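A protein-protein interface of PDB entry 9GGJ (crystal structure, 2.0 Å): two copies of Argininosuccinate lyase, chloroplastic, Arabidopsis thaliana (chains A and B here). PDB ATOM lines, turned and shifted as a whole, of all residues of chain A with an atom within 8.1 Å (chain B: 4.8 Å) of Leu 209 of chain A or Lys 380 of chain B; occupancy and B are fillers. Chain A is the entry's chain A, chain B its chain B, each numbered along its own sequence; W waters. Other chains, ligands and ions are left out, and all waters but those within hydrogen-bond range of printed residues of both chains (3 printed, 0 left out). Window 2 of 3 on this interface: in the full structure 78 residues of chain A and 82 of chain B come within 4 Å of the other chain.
O of Thr 207 of chain A is in hydrogen-bond range of N of Ser 439 of chain B, at 3.0 Å.
The backbone NH (N) of Gly 208 of chain A is in hydrogen-bond range of the side-chain carboxylate (OD2) of Asp 376 of chain B.
NZ of Lys 380 of chain B sits close to O of Gly 208 of chain A (3.3 Å).
The side-chain hydroxyl (OG) of Ser 439 of chain B sits at hydrogen-bond distance from the backbone carbonyl oxygen (O) of Gly 208 of chain A.
The backbone NH (N) of Leu 209 of chain A lies within hydrogen-bond range of the side-chain hydroxyl (OG1) of Thr 207 of chain A, 2.9 Å away.
Among the printed residues, merely in contact across the chains: Leu 209 of chain A with Asp 376 of chain B (3.6 Å), Thr 207 of chain A with Asp 376 of chain B (3.7 Å), Leu 209 of chain A with Lys 380 of chain B (3.8 Å) and Leu 209 of chain A with Val 379 of chain B (3.97 Å).
Of the printed residues of chain B, Thr 207 of chain A touches Asp 376 (3.7 Å) and Ser 439 (3.0 Å).
Printed residues of chain B within 4 Å of Gly 208 of chain A: Asp 376 (3.4 Å), Lys 380 (3.2 Å) and Ser 439 (3.3 Å).
Leu 209 of chain A touches three residues of chain B.
Of the printed residues of chain A, Asp 376 of chain B touches Thr 207 (3.7 Å), Gly 208 (3.4 Å) and Leu 209 (3.6 Å).
Printed residues of chain A within 4 Å of Val 379 of chain B: Leu 209 (3.97 Å).
Of chain A, only Gly 208 and Leu 209 come within 4 Å of Lys 380 of chain B.
Printed residues of chain A within 4 Å of Ser 439 of chain B: Thr 207 (3.0 Å) and Gly 208 (3.3 Å).
The nearest residue of chain B that does not touch Leu 209 of chain A is Ser 439 of chain B (4.3 Å).
The nearest printed residue of chain B that does not touch Thr 207 of chain A is Lys 380 of chain B (6.9 Å).
Of the 9 printed residues of chain B, 4 touch a printed residue of chain A.
Along chain A the printed residues that touch a printed residue of chain B span positions 207 to 209.
No position is printed for both chains.
Of the 8 pairs that touch across the chains among the printed residues, none has its exchanged pair printed and touching as well.
Water W1 bridges the side-chain hydroxyl of Thr 207 of chain A (2.5 Å) and the side-chain carboxylate of Asp 376 of chain B (2.7 Å).
Water W2 lies within hydrogen-bond range of the backbone carbonyl oxygen (O) of Leu 209 of chain A (2.5 Å) and the side-chain hydroxyl (OG) of Ser 439 of chain B (2.9 Å).
Water W3 lies within hydrogen-bond range of NZ of Lys 380 of chain B (2.9 Å) and O of Gly 208 of chain A (3.0 Å).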
ATOM      1  N   MET A  48     -17.932 -17.437 -24.036  1.00  0.00           N
ATOM      2  CA  MET A  48     -16.871 -17.589 -25.035  1.00  0.00           C
ATOM      3  C   MET A  48     -17.135 -18.819 -25.897  1.00  0.00           C
ATOM      4  O   MET A  48     -16.921 -18.772 -27.093  1.00  0.00           O
ATOM      5  CB  MET A  48     -15.475 -17.625 -24.405  1.00  0.00           C
ATOM      6  CG  MET A  48     -14.344 -17.980 -25.356  1.00  0.00           C
ATOM      7  SD  MET A  48     -14.136 -19.760 -25.582  1.00  0.00           S
ATOM      8  CE  MET A  48     -13.579 -20.425 -24.003  1.00  0.00           C
ATOM      9  N   LEU A  49     -17.603 -19.916 -25.305  1.00  0.00           N
ATOM     10  CA  LEU A  49     -17.816 -21.151 -26.041  1.00  0.00           C
ATOM     11  C   LEU A  49     -18.829 -20.904 -27.157  1.00  0.00           C
ATOM     12  O   LEU A  49     -18.654 -21.341 -28.294  1.00  0.00           O
ATOM     13  CB  LEU A  49     -18.310 -22.255 -25.101  1.00  0.00           C
ATOM     14  CG  LEU A  49     -17.339 -22.863 -24.079  1.00  0.00           C
ATOM     15  CD1 LEU A  49     -18.212 -23.819 -23.270  1.00  0.00           C
ATOM     16  CD2 LEU A  49     -16.130 -23.602 -24.681  1.00  0.00           C
ATOM     17  N   GLN A  52     -17.578 -18.946 -30.014  1.00  0.00           N
ATOM     18  CA  GLN A  52     -16.602 -19.636 -30.818  1.00  0.00           C
ATOM     19  C   GLN A  52     -17.222 -20.832 -31.521  1.00  0.00           C
ATOM     20  O   GLN A  52     -16.495 -21.572 -32.178  1.00  0.00           O
ATOM     21  CB  GLN A  52     -15.500 -20.109 -29.888  1.00  0.00           C
ATOM     22  CG  GLN A  52     -14.696 -18.966 -29.288  1.00  0.00           C
ATOM     23  CD  GLN A  52     -14.136 -18.041 -30.341  1.00  0.00           C
ATOM     24  OE1 GLN A  52     -14.680 -16.960 -30.586  1.00  0.00           O
ATOM     25  NE2 GLN A  52     -13.089 -18.498 -31.019  1.00  0.00           N
ATOM     26  N   GLY A  53     -18.538 -21.043 -31.338  1.00  0.00           N
ATOM     27  CA  GLY A  53     -19.245 -22.107 -32.042  1.00  0.00           C
ATOM     28  C   GLY A  53     -19.128 -23.485 -31.390  1.00  0.00           C
ATOM     29  O   GLY A  53     -19.533 -24.463 -31.992  1.00  0.00           O
ATOM     30  N   LEU A  54     -18.623 -23.583 -30.156  1.00  0.00           N
ATOM     31  CA  LEU A  54     -18.456 -24.885 -29.506  1.00  0.00           C
ATOM     32  C   LEU A  54     -19.716 -25.345 -28.773  1.00  0.00           C
ATOM     33  O   LEU A  54     -19.868 -26.526 -28.474  1.00  0.00           O
ATOM     34  CB  LEU A  54     -17.275 -24.821 -28.544  1.00  0.00           C
ATOM     35  CG  LEU A  54     -15.919 -24.805 -29.254  1.00  0.00           C
ATOM     36  CD1 LEU A  54     -14.860 -24.274 -28.351  1.00  0.00           C
ATOM     37  CD2 LEU A  54     -15.644 -26.224 -29.726  1.00  0.00           C
ATOM     38  N   HIS A 108     -18.236 -28.016 -19.314  1.00  0.00           N
ATOM     39  CA  HIS A 108     -16.893 -28.504 -19.064  1.00  0.00           C
ATOM     40  C   HIS A 108     -16.011 -28.503 -20.325  1.00  0.00           C
ATOM     41  O   HIS A 108     -14.795 -28.736 -20.244  1.00  0.00           O
ATOM     42  CB  HIS A 108     -16.937 -29.904 -18.435  1.00  0.00           C
ATOM     43  CG  HIS A 108     -15.722 -30.168 -17.620  1.00  0.00           C
ATOM     44  ND1 HIS A 108     -15.333 -29.294 -16.614  1.00  0.00           N
ATOM     45  CD2 HIS A 108     -14.785 -31.125 -17.689  1.00  0.00           C
ATOM     46  CE1 HIS A 108     -14.201 -29.727 -16.078  1.00  0.00           C
ATOM     47  NE2 HIS A 108     -13.851 -30.843 -16.726  1.00  0.00           N
ATOM     48  N   THR A 109     -16.611 -28.214 -21.489  1.00  0.00           N
ATOM     49  CA  THR A 109     -15.914 -28.185 -22.762  1.00  0.00           C
ATOM     50  C   THR A 109     -14.672 -27.299 -22.695  1.00  0.00           C
ATOM     51  O   THR A 109     -14.774 -26.098 -22.480  1.00  0.00           O
ATOM     52  CB  THR A 109     -16.833 -27.642 -23.848  1.00  0.00           C
ATOM     53  OG1 THR A 109     -17.984 -28.474 -23.926  1.00  0.00           O
ATOM     54  CG2 THR A 109     -16.148 -27.647 -25.196  1.00  0.00           C
ATOM     55  N   ALA A 110     -13.507 -27.894 -22.971  1.00  0.00           N
ATOM     56  CA  ALA A 110     -12.278 -27.143 -23.127  1.00  0.00           C
ATOM     57  C   ALA A 110     -11.903 -26.447 -21.834  1.00  0.00           C
ATOM     58  O   ALA A 110     -11.355 -25.348 -21.882  1.00  0.00           O
ATOM     59  CB  ALA A 110     -12.418 -26.125 -24.220  1.00  0.00           C
ATOM     60  N   ARG A 111     -12.186 -27.095 -20.697  1.00  0.00           N
ATOM     61  CA  ARG A 111     -11.779 -26.569 -19.408  1.00  0.00           C
ATOM     62  C   ARG A 111     -11.398 -27.730 -18.499  1.00  0.00           C
ATOM     63  O   ARG A 111     -11.961 -28.796 -18.636  1.00  0.00           O
ATOM     64  CB  ARG A 111     -12.993 -25.792 -18.881  1.00  0.00           C
ATOM     65  CG  ARG A 111     -12.700 -24.861 -17.721  1.00  0.00           C
ATOM     66  CD  ARG A 111     -13.922 -24.081 -17.240  1.00  0.00           C
ATOM     67  NE  ARG A 111     -14.965 -24.948 -16.678  1.00  0.00           N
ATOM     68  CZ  ARG A 111     -16.087 -24.514 -16.084  1.00  0.00           C
ATOM     69  NH1 ARG A 111     -16.299 -23.217 -15.954  1.00  0.00           N
ATOM     70  NH2 ARG A 111     -16.986 -25.375 -15.626  1.00  0.00           N
ATOM     71  N   GLY A 200      -8.160 -21.341 -19.841  1.00  0.00           N
ATOM     72  CA  GLY A 200      -7.912 -21.864 -21.165  1.00  0.00           C
ATOM     73  C   GLY A 200      -6.613 -22.637 -21.257  1.00  0.00           C
ATOM     74  O   GLY A 200      -6.255 -23.055 -22.331  1.00  0.00           O
ATOM     75  N   CYS A 202      -6.501 -25.436 -19.667  1.00  0.00           N
ATOM     76  CA  CYS A 202      -7.031 -26.782 -19.459  1.00  0.00           C
ATOM     77  C   CYS A 202      -6.170 -27.494 -18.416  1.00  0.00           C
ATOM     78  O   CYS A 202      -5.667 -26.836 -17.491  1.00  0.00           O
ATOM     79  CB  CYS A 202      -7.230 -27.500 -20.788  1.00  0.00           C
ATOM     80  SG  CYS A 202      -8.293 -26.530 -21.897  1.00  0.00           S
ATOM     81  N   GLY A 206      -3.067 -26.779 -22.584  1.00  0.00           N
ATOM     82  CA  GLY A 206      -3.963 -26.032 -23.462  1.00  0.00           C
ATOM     83  C   GLY A 206      -4.912 -26.983 -24.188  1.00  0.00           C
ATOM     84  O   GLY A 206      -5.139 -28.098 -23.717  1.00  0.00           O
ATOM     85  N   THR A 207      -5.454 -26.539 -25.331  1.00  0.00           N
ATOM     86  CA  THR A 207      -6.404 -27.328 -26.105  1.00  0.00           C
ATOM     87  C   THR A 207      -6.171 -27.128 -27.603  1.00  0.00           C
ATOM     88  O   THR A 207      -5.579 -26.141 -28.039  1.00  0.00           O
ATOM     89  CB  THR A 207      -7.839 -26.947 -25.705  1.00  0.00           C
ATOM     90  OG1 THR A 207      -8.737 -27.707 -26.515  1.00  0.00           O
ATOM     91  CG2 THR A 207      -8.140 -25.471 -25.903  1.00  0.00           C
ATOM     92  N   GLY A 208      -6.695 -28.083 -28.383  1.00  0.00           N
ATOM     93  CA  GLY A 208      -6.850 -27.905 -29.817  1.00  0.00           C
ATOM     94  C   GLY A 208      -8.188 -27.293 -30.236  1.00  0.00           C
ATOM     95  O   GLY A 208      -8.377 -27.065 -31.432  1.00  0.00           O
ATOM     96  N   LEU A 209      -9.098 -27.023 -29.274  1.00  0.00           N
ATOM     97  CA  LEU A 209     -10.423 -26.469 -29.566  1.00  0.00           C
ATOM     98  C   LEU A 209     -10.279 -24.977 -29.796  1.00  0.00           C
ATOM     99  O   LEU A 209      -9.372 -24.387 -29.229  1.00  0.00           O
ATOM    100  CB  LEU A 209     -11.449 -26.775 -28.473  1.00  0.00           C
ATOM    101  CG  LEU A 209     -11.726 -28.275 -28.325  1.00  0.00           C
ATOM    102  CD1 LEU A 209     -12.497 -28.571 -27.093  1.00  0.00           C
ATOM    103  CD2 LEU A 209     -12.448 -28.792 -29.554  1.00  0.00           C
ATOM    104  N   PRO A 210     -11.091 -24.373 -30.685  1.00  0.00           N
ATOM    105  CA  PRO A 210     -10.960 -22.958 -31.013  1.00  0.00           C
ATOM    106  C   PRO A 210     -11.603 -22.004 -30.004  1.00  0.00           C
ATOM    107  O   PRO A 210     -12.491 -21.205 -30.327  1.00  0.00           O
ATOM    108  CB  PRO A 210     -11.594 -22.923 -32.422  1.00  0.00           C
ATOM    109  CG  PRO A 210     -12.700 -23.947 -32.362  1.00  0.00           C
ATOM    110  CD  PRO A 210     -12.109 -25.055 -31.498  1.00  0.00           C
ATOM    111  N   ILE A 211     -11.110 -22.086 -28.758  1.00  0.00           N
ATOM    112  CA  ILE A 211     -11.456 -21.147 -27.716  1.00  0.00           C
ATOM    113  C   ILE A 211     -10.792 -19.816 -28.038  1.00  0.00           C
ATOM    114  O   ILE A 211      -9.949 -19.729 -28.930  1.00  0.00           O
ATOM    115  CB  ILE A 211     -11.011 -21.651 -26.337  1.00  0.00           C
ATOM    116  CG1 ILE A 211      -9.502 -21.734 -26.220  1.00  0.00           C
ATOM    117  CG2 ILE A 211     -11.685 -22.974 -26.002  1.00  0.00           C
ATOM    118  CD1 ILE A 211      -9.022 -22.211 -24.861  1.00  0.00           C
ATOM    119  N   ASP A 212     -11.204 -18.778 -27.306  1.00  0.00           N
ATOM    120  CA  ASP A 212     -10.573 -17.470 -27.361  1.00  0.00           C
ATOM    121  C   ASP A 212     -10.249 -17.079 -25.924  1.00  0.00           C
ATOM    122  O   ASP A 212     -11.138 -16.660 -25.169  1.00  0.00           O
ATOM    123  CB  ASP A 212     -11.454 -16.455 -28.077  1.00  0.00           C
ATOM    124  CG  ASP A 212     -10.861 -15.056 -28.225  1.00  0.00           C
ATOM    125  OD1 ASP A 212      -9.823 -14.779 -27.583  1.00  0.00           O
ATOM    126  OD2 ASP A 212     -11.431 -14.242 -28.993  1.00  0.00           O
ATOM    127  N   ARG A 213      -8.969 -17.196 -25.574  1.00  0.00           N
ATOM    128  CA  ARG A 213      -8.495 -16.814 -24.248  1.00  0.00           C
ATOM    129  C   ARG A 213      -8.492 -15.299 -24.039  1.00  0.00           C
ATOM    130  O   ARG A 213      -8.612 -14.865 -22.902  1.00  0.00           O
ATOM    131  CB  ARG A 213      -7.126 -17.441 -23.990  1.00  0.00           C
ATOM    132  CG  ARG A 213      -7.190 -18.961 -23.966  1.00  0.00           C
ATOM    133  CD  ARG A 213      -5.921 -19.605 -23.456  1.00  0.00           C
ATOM    134  NE  ARG A 213      -5.643 -19.223 -22.071  1.00  0.00           N
ATOM    135  CZ  ARG A 213      -4.463 -18.817 -21.623  1.00  0.00           C
ATOM    136  NH1 ARG A 213      -3.377 -18.919 -22.379  1.00  0.00           N
ATOM    137  NH2 ARG A 213      -4.321 -18.336 -20.402  1.00  0.00           N
ATOM    138  N   ASP B 376     -11.127 -34.086 -28.593  1.00  0.00           N
ATOM    139  CA  ASP B 376     -11.304 -32.784 -29.213  1.00  0.00           C
ATOM    140  C   ASP B 376     -11.731 -32.923 -30.673  1.00  0.00           C
ATOM    141  O   ASP B 376     -12.452 -32.058 -31.170  1.00  0.00           O
ATOM    142  CB  ASP B 376     -10.029 -31.962 -29.258  1.00  0.00           C
ATOM    143  CG  ASP B 376      -9.481 -31.450 -27.933  1.00  0.00           C
ATOM    144  OD1 ASP B 376     -10.237 -31.460 -26.920  1.00  0.00           O
ATOM    145  OD2 ASP B 376      -8.281 -31.040 -27.934  1.00  0.00           O
ATOM    146  N   TYR B 377     -11.227 -33.958 -31.374  1.00  0.00           N
ATOM    147  CA  TYR B 377     -11.631 -34.229 -32.749  1.00  0.00           C
ATOM    148  C   TYR B 377     -13.154 -34.413 -32.807  1.00  0.00           C
ATOM    149  O   TYR B 377     -13.825 -33.795 -33.628  1.00  0.00           O
ATOM    150  CB  TYR B 377     -10.855 -35.449 -33.254  1.00  0.00           C
ATOM    151  CG  TYR B 377     -11.470 -36.107 -34.488  1.00  0.00           C
ATOM    152  CD1 TYR B 377     -11.173 -35.635 -35.755  1.00  0.00           C
ATOM    153  CD2 TYR B 377     -12.339 -37.192 -34.391  1.00  0.00           C
ATOM    154  CE1 TYR B 377     -11.695 -36.245 -36.885  1.00  0.00           C
ATOM    155  CE2 TYR B 377     -12.889 -37.790 -35.512  1.00  0.00           C
ATOM    156  CZ  TYR B 377     -12.569 -37.310 -36.770  1.00  0.00           C
ATOM    157  OH  TYR B 377     -13.086 -37.836 -37.935  1.00  0.00           O
ATOM    158  N   LEU B 378     -13.686 -35.243 -31.905  1.00  0.00           N
ATOM    159  CA  LEU B 378     -15.107 -35.558 -31.802  1.00  0.00           C
ATOM    160  C   LEU B 378     -15.928 -34.310 -31.461  1.00  0.00           C
ATOM    161  O   LEU B 378     -16.996 -34.128 -32.021  1.00  0.00           O
ATOM    162  CB  LEU B 378     -15.299 -36.656 -30.752  1.00  0.00           C
ATOM    163  CG  LEU B 378     -14.942 -38.073 -31.202  1.00  0.00           C
ATOM    164  CD1 LEU B 378     -15.147 -39.110 -30.102  1.00  0.00           C
ATOM    165  CD2 LEU B 378     -15.773 -38.444 -32.424  1.00  0.00           C
ATOM    166  N   VAL B 379     -15.411 -33.438 -30.585  1.00  0.00           N
ATOM    167  CA  VAL B 379     -16.113 -32.214 -30.220  1.00  0.00           C
ATOM    168  C   VAL B 379     -16.201 -31.315 -31.445  1.00  0.00           C
ATOM    169  O   VAL B 379     -17.252 -30.726 -31.704  1.00  0.00           O
ATOM    170  CB  VAL B 379     -15.477 -31.468 -29.033  1.00  0.00           C
ATOM    171  CG1 VAL B 379     -16.112 -30.097 -28.775  1.00  0.00           C
ATOM    172  CG2 VAL B 379     -15.553 -32.286 -27.755  1.00  0.00           C
ATOM    173  N   LYS B 380     -15.113 -31.253 -32.222  1.00  0.00           N
ATOM    174  CA  LYS B 380     -15.076 -30.431 -33.426  1.00  0.00           C
ATOM    175  C   LYS B 380     -16.001 -30.987 -34.516  1.00  0.00           C
ATOM    176  O   LYS B 380     -16.481 -30.214 -35.330  1.00  0.00           O
ATOM    177  CB  LYS B 380     -13.667 -30.335 -34.025  1.00  0.00           C
ATOM    178  CG  LYS B 380     -12.648 -29.519 -33.246  1.00  0.00           C
ATOM    179  CD  LYS B 380     -11.229 -30.003 -33.554  1.00  0.00           C
ATOM    180  CE  LYS B 380     -10.149 -29.053 -33.141  1.00  0.00           C
ATOM    181  NZ  LYS B 380      -8.813 -29.610 -33.435  1.00  0.00           N
ATOM    182  N   LYS B 381     -16.247 -32.304 -34.539  1.00  0.00           N
ATOM    183  CA  LYS B 381     -17.247 -32.899 -35.424  1.00  0.00           C
ATOM    184  C   LYS B 381     -18.686 -32.740 -34.911  1.00  0.00           C
ATOM    185  O   LYS B 381     -19.624 -33.106 -35.602  1.00  0.00           O
ATOM    186  CB  LYS B 381     -17.090 -34.419 -35.554  1.00  0.00           C
ATOM    187  CG  LYS B 381     -15.858 -34.889 -36.259  1.00  0.00           C
ATOM    188  CD  LYS B 381     -15.701 -34.387 -37.677  1.00  0.00           C
ATOM    189  CE  LYS B 381     -14.542 -35.098 -38.293  1.00  0.00           C
ATOM    190  NZ  LYS B 381     -14.242 -34.472 -39.570  1.00  0.00           N
ATOM    191  N   GLY B 382     -18.865 -32.269 -33.680  1.00  0.00           N
ATOM    192  CA  GLY B 382     -20.169 -31.906 -33.148  1.00  0.00           C
ATOM    193  C   GLY B 382     -20.597 -32.754 -31.951  1.00  0.00           C
ATOM    194  O   GLY B 382     -21.727 -32.600 -31.500  1.00  0.00           O
ATOM    195  N   PHE B 428      -5.124 -37.015 -36.370  1.00  0.00           N
ATOM    196  CA  PHE B 428      -5.247 -36.492 -35.024  1.00  0.00           C
ATOM    197  C   PHE B 428      -4.596 -37.429 -34.003  1.00  0.00           C
ATOM    198  O   PHE B 428      -4.424 -37.002 -32.868  1.00  0.00           O
ATOM    199  CB  PHE B 428      -6.725 -36.226 -34.688  1.00  0.00           C
ATOM    200  CG  PHE B 428      -7.374 -35.048 -35.406  1.00  0.00           C
ATOM    201  CD1 PHE B 428      -7.705 -35.121 -36.756  1.00  0.00           C
ATOM    202  CD2 PHE B 428      -7.678 -33.885 -34.727  1.00  0.00           C
ATOM    203  CE1 PHE B 428      -8.307 -34.057 -37.412  1.00  0.00           C
ATOM    204  CE2 PHE B 428      -8.299 -32.819 -35.383  1.00  0.00           C
ATOM    205  CZ  PHE B 428      -8.621 -32.911 -36.727  1.00  0.00           C
ATOM    206  N   SER B 439      -3.513 -25.569 -30.146  1.00  0.00           N
ATOM    207  CA  SER B 439      -3.639 -24.338 -30.905  1.00  0.00           C
ATOM    208  C   SER B 439      -4.057 -23.140 -30.061  1.00  0.00           C
ATOM    209  O   SER B 439      -4.058 -22.032 -30.564  1.00  0.00           O
ATOM    210  CB  SER B 439      -4.581 -24.527 -32.071  1.00  0.00           C
ATOM    211  OG  SER B 439      -5.871 -24.919 -31.628  1.00  0.00           O
HETATM  212  O   HOH W   1      -9.211 -29.771 -25.147  1.00  0.00           O
HETATM  213  O   HOH W   2      -7.249 -23.114 -29.830  1.00  0.00           O
HETATM  214  O   HOH W   3      -6.314 -28.058 -33.306  1.00  0.00           O
